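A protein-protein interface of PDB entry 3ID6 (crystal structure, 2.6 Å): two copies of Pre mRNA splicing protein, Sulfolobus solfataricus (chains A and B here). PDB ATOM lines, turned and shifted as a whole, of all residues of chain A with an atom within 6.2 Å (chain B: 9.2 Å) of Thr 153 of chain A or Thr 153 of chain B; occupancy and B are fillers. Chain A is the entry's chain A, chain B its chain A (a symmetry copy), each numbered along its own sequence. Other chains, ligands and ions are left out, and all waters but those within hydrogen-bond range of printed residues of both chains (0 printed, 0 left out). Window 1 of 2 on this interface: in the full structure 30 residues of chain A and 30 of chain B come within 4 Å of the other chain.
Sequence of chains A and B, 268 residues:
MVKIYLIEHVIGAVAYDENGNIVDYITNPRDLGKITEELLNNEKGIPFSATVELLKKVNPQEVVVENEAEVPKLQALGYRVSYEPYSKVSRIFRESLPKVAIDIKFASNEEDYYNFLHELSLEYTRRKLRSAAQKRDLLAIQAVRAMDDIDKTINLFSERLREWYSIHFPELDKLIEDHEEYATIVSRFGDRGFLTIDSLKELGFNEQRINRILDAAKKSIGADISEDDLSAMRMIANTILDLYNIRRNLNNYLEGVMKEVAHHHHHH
NE of Arg 160 of chain B is in salt-bridge range of OD2 of Asp 149 of chain A (3.0 Å).
O of Asp 149 of chain A lies within hydrogen-bond range of OG1 of Thr 153 of chain A, 2.6 Å away.
The backbone carbonyl oxygen (O) of Asp 149 of chain B sits at hydrogen-bond distance from the side-chain hydroxyl (OG1) of Thr 153 of chain B (2.6 Å).
Among the printed residues, pairs that only touch across the chains: Asp 149 of chain A with Leu 156 of chain B (3.8 Å), Asp 149 of chain A with Phe 157 of chain B (3.7 Å), Ile 150 of chain A with Phe 157 of chain B (3.99 Å), Thr 153 of chain A with Thr 153 of chain B (3.4 Å), Thr 153 of chain A with Leu 156 of chain B (3.8 Å), Thr 153 of chain A with Phe 157 of chain B (3.3 Å), Leu 156 of chain A with Asp 149 of chain B (3.8 Å), Leu 156 of chain A with Thr 153 of chain B (3.8 Å), Phe 157 of chain A with Asp 149 of chain B (3.7 Å), Phe 157 of chain A with Ile 150 of chain B (3.99 Å), Phe 157 of chain A with Thr 153 of chain B (3.3 Å), Phe 157 of chain A with Leu 243 of chain B (3.96 Å), Leu 243 of chain A with Phe 157 of chain B (3.96 Å) and Leu 243 of chain A with Thr 239 of chain B (3.7 Å).
Of chain B, only Thr 153 (3.4 Å), Leu 156 (3.8 Å) and Phe 157 (3.3 Å) come within 4 Å of Thr 153 of chain A.
Of the printed residues of chain B, Phe 157 of chain A touches Asp 149, Ile 150, Thr 153 and Leu 243.
Printed residues of chain A within 4 Å of Ile 150 of chain B: Phe 157 (3.99 Å).
Thr 153 of chain B touches three residues of chain A.
Printed residues of chain A within 4 Å of Phe 157 of chain B: Asp 149, Ile 150, Thr 153 and Leu 243.
The nearest printed residue of chain B that does not touch Ile 150 of chain A is Ile 236 of chain B (4.5 Å).
Of the 23 printed residues of chain B, 8 touch a printed residue of chain A.
Hydrophobic or aromatic side chains of chain B that line the printed part of chain A: Leu 156, Phe 157 and Leu 243.
Along chain A the printed residues that touch a printed residue of chain B span positions 149 to 243.
Among the printed residues, 15 pairs touch across the chains.
Among the printed residues, Asp or Glu carboxylates within 4 Å of a Lys or Arg side-chain nitrogen of the other chain: Asp 149 of chain A with Arg 160 of chain B.
Ile 150 of chain A touches Phe 157 of chain B, and with the chains exchanged Phe 157 of chain A touches Ile 150 of chain B.
Thr 153 of chain A touches its own counterpart, Thr 153 of chain B.
Thr 153 of chain A touches Leu 156 of chain B, and with the chains exchanged Leu 156 of chain A touches Thr 153 of chain B.
Phe 157 of chain A touches Leu 243 of chain B, and with the chains exchanged Leu 243 of chain A touches Phe 157 of chain B.
13 positions are printed for both chains.
Of the 15 pairs that touch across the chains among the printed residues, 13 have their exchanged pair printed and touching as well.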
ATOM      1  N   ASP A 148     -17.150 -24.345  26.942  1.00  0.00           N
ATOM      2  CA  ASP A 148     -16.095 -23.330  26.963  1.00  0.00           C
ATOM      3  C   ASP A 148     -15.068 -23.568  25.848  1.00  0.00           C
ATOM      4  O   ASP A 148     -14.669 -22.632  25.141  1.00  0.00           O
ATOM      5  CB  ASP A 148     -15.414 -23.290  28.335  1.00  0.00           C
ATOM      6  CG  ASP A 148     -16.420 -23.132  29.481  1.00  0.00           C
ATOM      7  OD1 ASP A 148     -17.329 -22.267  29.366  1.00  0.00           O
ATOM      8  OD2 ASP A 148     -16.318 -23.880  30.496  1.00  0.00           O
ATOM      9  N   ASP A 149     -14.673 -24.833  25.683  1.00  0.00           N
ATOM     10  CA  ASP A 149     -13.744 -25.247  24.636  1.00  0.00           C
ATOM     11  C   ASP A 149     -14.279 -24.949  23.258  1.00  0.00           C
ATOM     12  O   ASP A 149     -13.543 -24.483  22.404  1.00  0.00           O
ATOM     13  CB  ASP A 149     -13.422 -26.732  24.775  1.00  0.00           C
ATOM     14  CG  ASP A 149     -12.608 -27.026  26.024  1.00  0.00           C
ATOM     15  OD1 ASP A 149     -11.909 -26.097  26.485  1.00  0.00           O
ATOM     16  OD2 ASP A 149     -12.670 -28.173  26.551  1.00  0.00           O
ATOM     17  N   ILE A 150     -15.568 -25.207  23.065  1.00  0.00           N
ATOM     18  CA  ILE A 150     -16.268 -24.907  21.826  1.00  0.00           C
ATOM     19  C   ILE A 150     -16.390 -23.393  21.571  1.00  0.00           C
ATOM     20  O   ILE A 150     -16.215 -22.939  20.435  1.00  0.00           O
ATOM     21  CB  ILE A 150     -17.659 -25.576  21.817  1.00  0.00           C
ATOM     22  CG1 ILE A 150     -17.504 -27.097  21.738  1.00  0.00           C
ATOM     23  CG2 ILE A 150     -18.514 -25.059  20.675  1.00  0.00           C
ATOM     24  CD1 ILE A 150     -18.745 -27.869  22.106  1.00  0.00           C
ATOM     25  N   ASP A 151     -16.693 -22.621  22.616  1.00  0.00           N
ATOM     26  CA  ASP A 151     -16.740 -21.160  22.503  1.00  0.00           C
ATOM     27  C   ASP A 151     -15.419 -20.640  21.983  1.00  0.00           C
ATOM     28  O   ASP A 151     -15.368 -19.973  20.945  1.00  0.00           O
ATOM     29  CB  ASP A 151     -17.026 -20.494  23.854  1.00  0.00           C
ATOM     30  CG  ASP A 151     -18.458 -20.665  24.309  1.00  0.00           C
ATOM     31  OD1 ASP A 151     -19.252 -21.347  23.611  1.00  0.00           O
ATOM     32  OD2 ASP A 151     -18.796 -20.111  25.385  1.00  0.00           O
ATOM     33  N   LYS A 152     -14.358 -20.963  22.714  1.00  0.00           N
ATOM     34  CA  LYS A 152     -12.990 -20.584  22.362  1.00  0.00           C
ATOM     35  C   LYS A 152     -12.639 -20.969  20.911  1.00  0.00           C
ATOM     36  O   LYS A 152     -12.076 -20.156  20.175  1.00  0.00           O
ATOM     37  CB  LYS A 152     -12.027 -21.234  23.359  1.00  0.00           C
ATOM     38  CG  LYS A 152     -10.577 -20.855  23.240  1.00  0.00           C
ATOM     39  CD  LYS A 152      -9.690 -21.785  24.095  1.00  0.00           C
ATOM     40  CE  LYS A 152      -9.938 -21.638  25.600  1.00  0.00           C
ATOM     41  NZ  LYS A 152      -9.318 -22.748  26.405  1.00  0.00           N
ATOM     42  N   THR A 153     -13.009 -22.187  20.515  1.00  0.00           N
ATOM     43  CA  THR A 153     -12.778 -22.704  19.177  1.00  0.00           C
ATOM     44  C   THR A 153     -13.565 -21.925  18.111  1.00  0.00           C
ATOM     45  O   THR A 153     -13.048 -21.656  17.025  1.00  0.00           O
ATOM     46  CB  THR A 153     -13.127 -24.217  19.092  1.00  0.00           C
ATOM     47  OG1 THR A 153     -12.390 -24.951  20.074  1.00  0.00           O
ATOM     48  CG2 THR A 153     -12.783 -24.776  17.748  1.00  0.00           C
ATOM     49  N   ILE A 154     -14.811 -21.570  18.423  1.00  0.00           N
ATOM     50  CA  ILE A 154     -15.643 -20.788  17.510  1.00  0.00           C
ATOM     51  C   ILE A 154     -14.943 -19.461  17.239  1.00  0.00           C
ATOM     52  O   ILE A 154     -14.768 -19.072  16.089  1.00  0.00           O
ATOM     53  CB  ILE A 154     -17.124 -20.616  18.041  1.00  0.00           C
ATOM     54  CG1 ILE A 154     -17.967 -21.868  17.734  1.00  0.00           C
ATOM     55  CG2 ILE A 154     -17.826 -19.371  17.445  1.00  0.00           C
ATOM     56  CD1 ILE A 154     -19.274 -21.957  18.545  1.00  0.00           C
ATOM     57  N   ASN A 155     -14.486 -18.786  18.285  1.00  0.00           N
ATOM     58  CA  ASN A 155     -13.792 -17.517  18.077  1.00  0.00           C
ATOM     59  C   ASN A 155     -12.540 -17.687  17.248  1.00  0.00           C
ATOM     60  O   ASN A 155     -12.231 -16.832  16.416  1.00  0.00           O
ATOM     61  CB  ASN A 155     -13.482 -16.821  19.399  1.00  0.00           C
ATOM     62  CG  ASN A 155     -14.740 -16.394  20.135  1.00  0.00           C
ATOM     63  OD1 ASN A 155     -14.750 -16.301  21.353  1.00  0.00           O
ATOM     64  ND2 ASN A 155     -15.803 -16.132  19.396  1.00  0.00           N
ATOM     65  N   LEU A 156     -11.828 -18.792  17.468  1.00  0.00           N
ATOM     66  CA  LEU A 156     -10.586 -19.067  16.755  1.00  0.00           C
ATOM     67  C   LEU A 156     -10.865 -19.249  15.265  1.00  0.00           C
ATOM     68  O   LEU A 156     -10.341 -18.490  14.452  1.00  0.00           O
ATOM     69  CB  LEU A 156      -9.878 -20.294  17.341  1.00  0.00           C
ATOM     70  CG  LEU A 156      -8.490 -20.712  16.816  1.00  0.00           C
ATOM     71  CD1 LEU A 156      -7.366 -19.664  17.112  1.00  0.00           C
ATOM     72  CD2 LEU A 156      -8.115 -22.090  17.405  1.00  0.00           C
ATOM     73  N   PHE A 157     -11.725 -20.209  14.918  1.00  0.00           N
ATOM     74  CA  PHE A 157     -11.997 -20.546  13.525  1.00  0.00           C
ATOM     75  C   PHE A 157     -12.656 -19.410  12.792  1.00  0.00           C
ATOM     76  O   PHE A 157     -12.456 -19.230  11.597  1.00  0.00           O
ATOM     77  CB  PHE A 157     -12.897 -21.788  13.408  1.00  0.00           C
ATOM     78  CG  PHE A 157     -12.197 -23.093  13.687  1.00  0.00           C
ATOM     79  CD1 PHE A 157     -12.932 -24.248  13.909  1.00  0.00           C
ATOM     80  CD2 PHE A 157     -10.813 -23.173  13.750  1.00  0.00           C
ATOM     81  CE1 PHE A 157     -12.293 -25.476  14.183  1.00  0.00           C
ATOM     82  CE2 PHE A 157     -10.167 -24.396  14.030  1.00  0.00           C
ATOM     83  CZ  PHE A 157     -10.911 -25.550  14.233  1.00  0.00           C
ATOM     84  N   SER A 158     -13.456 -18.639  13.505  1.00  0.00           N
ATOM     85  CA  SER A 158     -14.237 -17.626  12.843  1.00  0.00           C
ATOM     86  C   SER A 158     -13.373 -16.400  12.577  1.00  0.00           C
ATOM     87  O   SER A 158     -13.594 -15.686  11.607  1.00  0.00           O
ATOM     88  CB  SER A 158     -15.505 -17.315  13.629  1.00  0.00           C
ATOM     89  OG  SER A 158     -15.350 -16.109  14.340  1.00  0.00           O
ATOM     90  N   ILE A 240     -17.698 -24.358  11.767  1.00  0.00           N
ATOM     91  CA  ILE A 240     -18.237 -23.360  12.703  1.00  0.00           C
ATOM     92  C   ILE A 240     -19.708 -23.609  12.918  1.00  0.00           C
ATOM     93  O   ILE A 240     -20.171 -23.643  14.056  1.00  0.00           O
ATOM     94  CB  ILE A 240     -18.018 -21.906  12.230  1.00  0.00           C
ATOM     95  CG1 ILE A 240     -16.512 -21.592  12.205  1.00  0.00           C
ATOM     96  CG2 ILE A 240     -18.812 -20.899  13.094  1.00  0.00           C
ATOM     97  CD1 ILE A 240     -16.141 -20.368  11.379  1.00  0.00           C
ATOM     98  N   LEU A 243     -20.197 -26.707  15.131  1.00  0.00           N
ATOM     99  CA  LEU A 243     -19.927 -26.382  16.519  1.00  0.00           C
ATOM    100  C   LEU A 243     -21.044 -25.591  17.218  1.00  0.00           C
ATOM    101  O   LEU A 243     -21.304 -25.829  18.400  1.00  0.00           O
ATOM    102  CB  LEU A 243     -18.593 -25.645  16.667  1.00  0.00           C
ATOM    103  CG  LEU A 243     -17.277 -26.308  16.239  1.00  0.00           C
ATOM    104  CD1 LEU A 243     -16.151 -25.281  16.362  1.00  0.00           C
ATOM    105  CD2 LEU A 243     -16.950 -27.628  16.998  1.00  0.00           C
ATOM    106  N   ARG B 145      -2.422 -21.749   8.062  1.00  0.00           N
ATOM    107  CA  ARG B 145      -2.722 -21.277   9.410  1.00  0.00           C
ATOM    108  C   ARG B 145      -3.971 -21.948   9.968  1.00  0.00           C
ATOM    109  O   ARG B 145      -4.048 -22.228  11.169  1.00  0.00           O
ATOM    110  CB  ARG B 145      -2.837 -19.756   9.437  1.00  0.00           C
ATOM    111  CG  ARG B 145      -1.507 -19.051   9.387  1.00  0.00           C
ATOM    112  CD  ARG B 145      -1.713 -17.543   9.300  1.00  0.00           C
ATOM    113  NE  ARG B 145      -0.673 -16.804  10.014  1.00  0.00           N
ATOM    114  CZ  ARG B 145       0.037 -15.805   9.497  1.00  0.00           C
ATOM    115  NH1 ARG B 145      -0.187 -15.389   8.253  1.00  0.00           N
ATOM    116  NH2 ARG B 145       0.962 -15.203  10.239  1.00  0.00           N
ATOM    117  N   ALA B 146      -4.933 -22.213   9.088  1.00  0.00           N
ATOM    118  CA  ALA B 146      -6.110 -22.992   9.456  1.00  0.00           C
ATOM    119  C   ALA B 146      -5.707 -24.400   9.908  1.00  0.00           C
ATOM    120  O   ALA B 146      -6.281 -24.927  10.849  1.00  0.00           O
ATOM    121  CB  ALA B 146      -7.131 -23.037   8.314  1.00  0.00           C
ATOM    122  N   MET B 147      -4.704 -24.996   9.270  1.00  0.00           N
ATOM    123  CA  MET B 147      -4.214 -26.302   9.712  1.00  0.00           C
ATOM    124  C   MET B 147      -3.615 -26.232  11.110  1.00  0.00           C
ATOM    125  O   MET B 147      -3.804 -27.142  11.908  1.00  0.00           O
ATOM    126  CB  MET B 147      -3.213 -26.904   8.716  1.00  0.00           C
ATOM    127  CG  MET B 147      -3.868 -27.363   7.414  1.00  0.00           C
ATOM    128  SD  MET B 147      -2.700 -27.862   6.126  1.00  0.00           S
ATOM    129  CE  MET B 147      -1.974 -29.336   6.852  1.00  0.00           C
ATOM    130  N   ASP B 148      -2.889 -25.153  11.401  1.00  0.00           N
ATOM    131  CA  ASP B 148      -2.379 -24.901  12.750  1.00  0.00           C
ATOM    132  C   ASP B 148      -3.523 -24.759  13.764  1.00  0.00           C
ATOM    133  O   ASP B 148      -3.478 -25.336  14.859  1.00  0.00           O
ATOM    134  CB  ASP B 148      -1.478 -23.662  12.763  1.00  0.00           C
ATOM    135  CG  ASP B 148      -0.368 -23.736  11.708  1.00  0.00           C
ATOM    136  OD1 ASP B 148       0.284 -24.808  11.599  1.00  0.00           O
ATOM    137  OD2 ASP B 148      -0.153 -22.731  10.971  1.00  0.00           O
ATOM    138  N   ASP B 149      -4.556 -24.010  13.369  1.00  0.00           N
ATOM    139  CA  ASP B 149      -5.752 -23.812  14.182  1.00  0.00           C
ATOM    140  C   ASP B 149      -6.457 -25.113  14.475  1.00  0.00           C
ATOM    141  O   ASP B 149      -6.891 -25.335  15.594  1.00  0.00           O
ATOM    142  CB  ASP B 149      -6.700 -22.834  13.495  1.00  0.00           C
ATOM    143  CG  ASP B 149      -6.135 -21.424  13.453  1.00  0.00           C
ATOM    144  OD1 ASP B 149      -5.302 -21.113  14.333  1.00  0.00           O
ATOM    145  OD2 ASP B 149      -6.509 -20.630  12.544  1.00  0.00           O
ATOM    146  N   ILE B 150      -6.544 -25.969  13.463  1.00  0.00           N
ATOM    147  CA  ILE B 150      -7.118 -27.300  13.587  1.00  0.00           C
ATOM    148  C   ILE B 150      -6.269 -28.225  14.478  1.00  0.00           C
ATOM    149  O   ILE B 150      -6.818 -28.981  15.287  1.00  0.00           O
ATOM    150  CB  ILE B 150      -7.329 -27.927  12.192  1.00  0.00           C
ATOM    151  CG1 ILE B 150      -8.430 -27.171  11.444  1.00  0.00           C
ATOM    152  CG2 ILE B 150      -7.661 -29.404  12.296  1.00  0.00           C
ATOM    153  CD1 ILE B 150      -8.463 -27.431   9.959  1.00  0.00           C
ATOM    154  N   ASP B 151      -4.945 -28.171  14.327  1.00  0.00           N
ATOM    155  CA  ASP B 151      -4.041 -28.939  15.189  1.00  0.00           C
ATOM    156  C   ASP B 151      -4.300 -28.599  16.640  1.00  0.00           C
ATOM    157  O   ASP B 151      -4.613 -29.479  17.448  1.00  0.00           O
ATOM    158  CB  ASP B 151      -2.570 -28.646  14.877  1.00  0.00           C
ATOM    159  CG  ASP B 151      -2.106 -29.258  13.575  1.00  0.00           C
ATOM    160  OD1 ASP B 151      -2.928 -29.884  12.857  1.00  0.00           O
ATOM    161  OD2 ASP B 151      -0.899 -29.108  13.260  1.00  0.00           O
ATOM    162  N   LYS B 152      -4.172 -27.314  16.950  1.00  0.00           N
ATOM    163  CA  LYS B 152      -4.411 -26.779  18.291  1.00  0.00           C
ATOM    164  C   LYS B 152      -5.778 -27.217  18.852  1.00  0.00           C
ATOM    165  O   LYS B 152      -5.866 -27.645  20.004  1.00  0.00           O
ATOM    166  CB  LYS B 152      -4.292 -25.255  18.241  1.00  0.00           C
ATOM    167  CG  LYS B 152      -4.378 -24.529  19.555  1.00  0.00           C
ATOM    168  CD  LYS B 152      -4.535 -23.008  19.338  1.00  0.00           C
ATOM    169  CE  LYS B 152      -3.306 -22.361  18.693  1.00  0.00           C
ATOM    170  NZ  LYS B 152      -3.573 -20.966  18.196  1.00  0.00           N
ATOM    171  N   THR B 153      -6.815 -27.137  18.015  1.00  0.00           N
ATOM    172  CA  THR B 153      -8.168 -27.529  18.372  1.00  0.00           C
ATOM    173  C   THR B 153      -8.281 -29.036  18.649  1.00  0.00           C
ATOM    174  O   THR B 153      -8.977 -29.450  19.579  1.00  0.00           O
ATOM    175  CB  THR B 153      -9.180 -27.117  17.265  1.00  0.00           C
ATOM    176  OG1 THR B 153      -9.090 -25.713  17.008  1.00  0.00           O
ATOM    177  CG2 THR B 153     -10.586 -27.417  17.680  1.00  0.00           C
ATOM    178  N   ILE B 154      -7.602 -29.849  17.842  1.00  0.00           N
ATOM    179  CA  ILE B 154      -7.595 -31.299  18.032  1.00  0.00           C
ATOM    180  C   ILE B 154      -7.025 -31.598  19.415  1.00  0.00           C
ATOM    181  O   ILE B 154      -7.628 -32.333  20.190  1.00  0.00           O
ATOM    182  CB  ILE B 154      -6.838 -32.057  16.867  1.00  0.00           C
ATOM    183  CG1 ILE B 154      -7.750 -32.225  15.637  1.00  0.00           C
ATOM    184  CG2 ILE B 154      -6.314 -33.446  17.307  1.00  0.00           C
ATOM    185  CD1 ILE B 154      -6.996 -32.583  14.343  1.00  0.00           C
ATOM    186  N   ASN B 155      -5.898 -30.991  19.756  1.00  0.00           N
ATOM    187  CA  ASN B 155      -5.320 -31.231  21.077  1.00  0.00           C
ATOM    188  C   ASN B 155      -6.252 -30.802  22.188  1.00  0.00           C
ATOM    189  O   ASN B 155      -6.336 -31.475  23.216  1.00  0.00           O
ATOM    190  CB  ASN B 155      -3.953 -30.570  21.224  1.00  0.00           C
ATOM    191  CG  ASN B 155      -2.917 -31.176  20.295  1.00  0.00           C
ATOM    192  OD1 ASN B 155      -1.972 -30.513  19.895  1.00  0.00           O
ATOM    193  ND2 ASN B 155      -3.091 -32.440  19.950  1.00  0.00           N
ATOM    194  N   LEU B 156      -6.955 -29.690  21.974  1.00  0.00           N
ATOM    195  CA  LEU B 156      -7.871 -29.151  22.973  1.00  0.00           C
ATOM    196  C   LEU B 156      -9.022 -30.125  23.212  1.00  0.00           C
ATOM    197  O   LEU B 156      -9.193 -30.600  24.333  1.00  0.00           O
ATOM    198  CB  LEU B 156      -8.390 -27.771  22.553  1.00  0.00           C
ATOM    199  CG  LEU B 156      -9.291 -26.959  23.504  1.00  0.00           C
ATOM    200  CD1 LEU B 156      -8.572 -26.515  24.822  1.00  0.00           C
ATOM    201  CD2 LEU B 156      -9.851 -25.730  22.753  1.00  0.00           C
ATOM    202  N   PHE B 157      -9.764 -30.463  22.155  1.00  0.00           N
ATOM    203  CA  PHE B 157     -10.949 -31.305  22.272  1.00  0.00           C
ATOM    204  C   PHE B 157     -10.605 -32.696  22.729  1.00  0.00           C
ATOM    205  O   PHE B 157     -11.384 -33.344  23.418  1.00  0.00           O
ATOM    206  CB  PHE B 157     -11.707 -31.404  20.937  1.00  0.00           C
ATOM    207  CG  PHE B 157     -12.500 -30.174  20.577  1.00  0.00           C
ATOM    208  CD1 PHE B 157     -12.983 -30.006  19.289  1.00  0.00           C
ATOM    209  CD2 PHE B 157     -12.749 -29.176  21.509  1.00  0.00           C
ATOM    210  CE1 PHE B 157     -13.717 -28.854  18.931  1.00  0.00           C
ATOM    211  CE2 PHE B 157     -13.476 -28.018  21.158  1.00  0.00           C
ATOM    212  CZ  PHE B 157     -13.971 -27.867  19.869  1.00  0.00           C
ATOM    213  N   SER B 158      -9.435 -33.168  22.341  1.00  0.00           N
ATOM    214  CA  SER B 158      -9.101 -34.542  22.612  1.00  0.00           C
ATOM    215  C   SER B 158      -8.625 -34.683  24.051  1.00  0.00           C
ATOM    216  O   SER B 158      -8.810 -35.726  24.665  1.00  0.00           O
ATOM    217  CB  SER B 158      -8.104 -35.072  21.588  1.00  0.00           C
ATOM    218  OG  SER B 158      -6.811 -35.107  22.145  1.00  0.00           O
ATOM    219  N   GLU B 159      -8.054 -33.619  24.603  1.00  0.00           N
ATOM    220  CA  GLU B 159      -7.759 -33.584  26.040  1.00  0.00           C
ATOM    221  C   GLU B 159      -9.033 -33.476  26.894  1.00  0.00           C
ATOM    222  O   GLU B 159      -9.073 -33.997  28.015  1.00  0.00           O
ATOM    223  CB  GLU B 159      -6.667 -32.547  26.377  1.00  0.00           C
ATOM    224  CG  GLU B 159      -5.246 -33.155  26.088  1.00  0.00           C
ATOM    225  CD  GLU B 159      -4.109 -32.142  25.879  1.00  0.00           C
ATOM    226  OE1 GLU B 159      -3.504 -31.693  26.898  1.00  0.00           O
ATOM    227  OE2 GLU B 159      -3.778 -31.840  24.693  1.00  0.00           O
ATOM    228  N   ARG B 160     -10.085 -32.867  26.329  1.00  0.00           N
ATOM    229  CA  ARG B 160     -11.400 -32.798  26.972  1.00  0.00           C
ATOM    230  C   ARG B 160     -12.107 -34.164  26.968  1.00  0.00           C
ATOM    231  O   ARG B 160     -12.677 -34.597  27.978  1.00  0.00           O
ATOM    232  CB  ARG B 160     -12.266 -31.742  26.283  1.00  0.00           C
ATOM    233  CG  ARG B 160     -13.719 -31.656  26.757  1.00  0.00           C
ATOM    234  CD  ARG B 160     -13.810 -31.384  28.237  1.00  0.00           C
ATOM    235  NE  ARG B 160     -12.923 -30.284  28.612  1.00  0.00           N
ATOM    236  CZ  ARG B 160     -12.266 -30.196  29.768  1.00  0.00           C
ATOM    237  NH1 ARG B 160     -11.493 -29.149  29.990  1.00  0.00           N
ATOM    238  NH2 ARG B 160     -12.386 -31.137  30.699  1.00  0.00           N
ATOM    239  N   LEU B 161     -12.063 -34.826  25.817  1.00  0.00           N
ATOM    240  CA  LEU B 161     -12.616 -36.155  25.646  1.00  0.00           C
ATOM    241  C   LEU B 161     -11.967 -37.165  26.600  1.00  0.00           C
ATOM    242  O   LEU B 161     -12.672 -37.932  27.265  1.00  0.00           O
ATOM    243  CB  LEU B 161     -12.396 -36.603  24.214  1.00  0.00           C
ATOM    244  CG  LEU B 161     -13.402 -37.505  23.497  1.00  0.00           C
ATOM    245  CD1 LEU B 161     -12.646 -38.471  22.558  1.00  0.00           C
ATOM    246  CD2 LEU B 161     -14.345 -38.266  24.434  1.00  0.00           C
ATOM    247  N   HIS B 179      -4.632 -39.442  19.067  1.00  0.00           N
ATOM    248  CA  HIS B 179      -5.899 -38.787  19.324  1.00  0.00           C
ATOM    249  C   HIS B 179      -7.013 -39.295  18.427  1.00  0.00           C
ATOM    250  O   HIS B 179      -8.158 -39.388  18.854  1.00  0.00           O
ATOM    251  CB  HIS B 179      -5.756 -37.262  19.229  1.00  0.00           C
ATOM    252  CG  HIS B 179      -5.017 -36.665  20.383  1.00  0.00           C
ATOM    253  ND1 HIS B 179      -4.235 -35.538  20.269  1.00  0.00           N
ATOM    254  CD2 HIS B 179      -4.921 -37.060  21.680  1.00  0.00           C
ATOM    255  CE1 HIS B 179      -3.702 -35.255  21.447  1.00  0.00           C
ATOM    256  NE2 HIS B 179      -4.108 -36.160  22.320  1.00  0.00           N
ATOM    257  N   ILE B 236     -18.231 -34.658  20.945  1.00  0.00           N
ATOM    258  CA  ILE B 236     -16.823 -34.239  20.926  1.00  0.00           C
ATOM    259  C   ILE B 236     -15.967 -35.192  20.091  1.00  0.00           C
ATOM    260  O   ILE B 236     -15.183 -34.750  19.242  1.00  0.00           O
ATOM    261  CB  ILE B 236     -16.248 -34.022  22.356  1.00  0.00           C
ATOM    262  CG1 ILE B 236     -16.539 -32.595  22.848  1.00  0.00           C
ATOM    263  CG2 ILE B 236     -14.744 -34.153  22.370  1.00  0.00           C
ATOM    264  CD1 ILE B 236     -17.989 -32.196  22.919  1.00  0.00           C
ATOM    265  N   THR B 239     -16.535 -34.700  16.340  1.00  0.00           N
ATOM    266  CA  THR B 239     -15.942 -33.442  15.934  1.00  0.00           C
ATOM    267  C   THR B 239     -14.445 -33.616  15.704  1.00  0.00           C
ATOM    268  O   THR B 239     -13.913 -33.059  14.747  1.00  0.00           O
ATOM    269  CB  THR B 239     -16.199 -32.328  16.977  1.00  0.00           C
ATOM    270  OG1 THR B 239     -17.605 -32.083  17.075  1.00  0.00           O
ATOM    271  CG2 THR B 239     -15.527 -31.042  16.571  1.00  0.00           C
ATOM    272  N   ILE B 240     -13.776 -34.394  16.564  1.00  0.00           N
ATOM    273  CA  ILE B 240     -12.338 -34.665  16.414  1.00  0.00           C
ATOM    274  C   ILE B 240     -12.093 -35.408  15.126  1.00  0.00           C
ATOM    275  O   ILE B 240     -11.213 -35.036  14.354  1.00  0.00           O
ATOM    276  CB  ILE B 240     -11.746 -35.463  17.597  1.00  0.00           C
ATOM    277  CG1 ILE B 240     -11.816 -34.615  18.879  1.00  0.00           C
ATOM    278  CG2 ILE B 240     -10.311 -35.950  17.295  1.00  0.00           C
ATOM    279  CD1 ILE B 240     -11.661 -35.412  20.167  1.00  0.00           C
ATOM    280  N   LEU B 243     -12.478 -33.017  12.147  1.00  0.00           N
ATOM    281  CA  LEU B 243     -11.304 -32.173  12.024  1.00  0.00           C
ATOM    282  C   LEU B 243     -10.076 -32.874  11.422  1.00  0.00           C
ATOM    283  O   LEU B 243      -9.334 -32.247  10.662  1.00  0.00           O
ATOM    284  CB  LEU B 243     -10.938 -31.534  13.366  1.00  0.00           C
ATOM    285  CG  LEU B 243     -11.919 -30.600  14.087  1.00  0.00           C
ATOM    286  CD1 LEU B 243     -11.340 -30.248  15.457  1.00  0.00           C
ATOM    287  CD2 LEU B 243     -12.309 -29.331  13.271  1.00  0.00           C
ATOM    288  N   TYR B 244      -9.844 -34.146  11.758  1.00  0.00           N
ATOM    289  CA  TYR B 244      -8.786 -34.914  11.084  1.00  0.00           C
ATOM    290  C   TYR B 244      -9.077 -34.959   9.599  1.00  0.00           C
ATOM    291  O   TYR B 244      -8.186 -34.783   8.767  1.00  0.00           O
ATOM    292  CB  TYR B 244      -8.650 -36.343  11.635  1.00  0.00           C
ATOM    293  CG  TYR B 244      -7.676 -36.450  12.793  1.00  0.00           C
ATOM    294  CD1 TYR B 244      -8.120 -36.435  14.112  1.00  0.00           C
ATOM    295  CD2 TYR B 244      -6.305 -36.546  12.563  1.00  0.00           C
ATOM    296  CE1 TYR B 244      -7.214 -36.528  15.184  1.00  0.00           C
ATOM    297  CE2 TYR B 244      -5.387 -36.633  13.615  1.00  0.00           C
ATOM    298  CZ  TYR B 244      -5.844 -36.631  14.928  1.00  0.00           C
ATOM    299  OH  TYR B 244      -4.927 -36.716  15.969  1.00  0.00           O
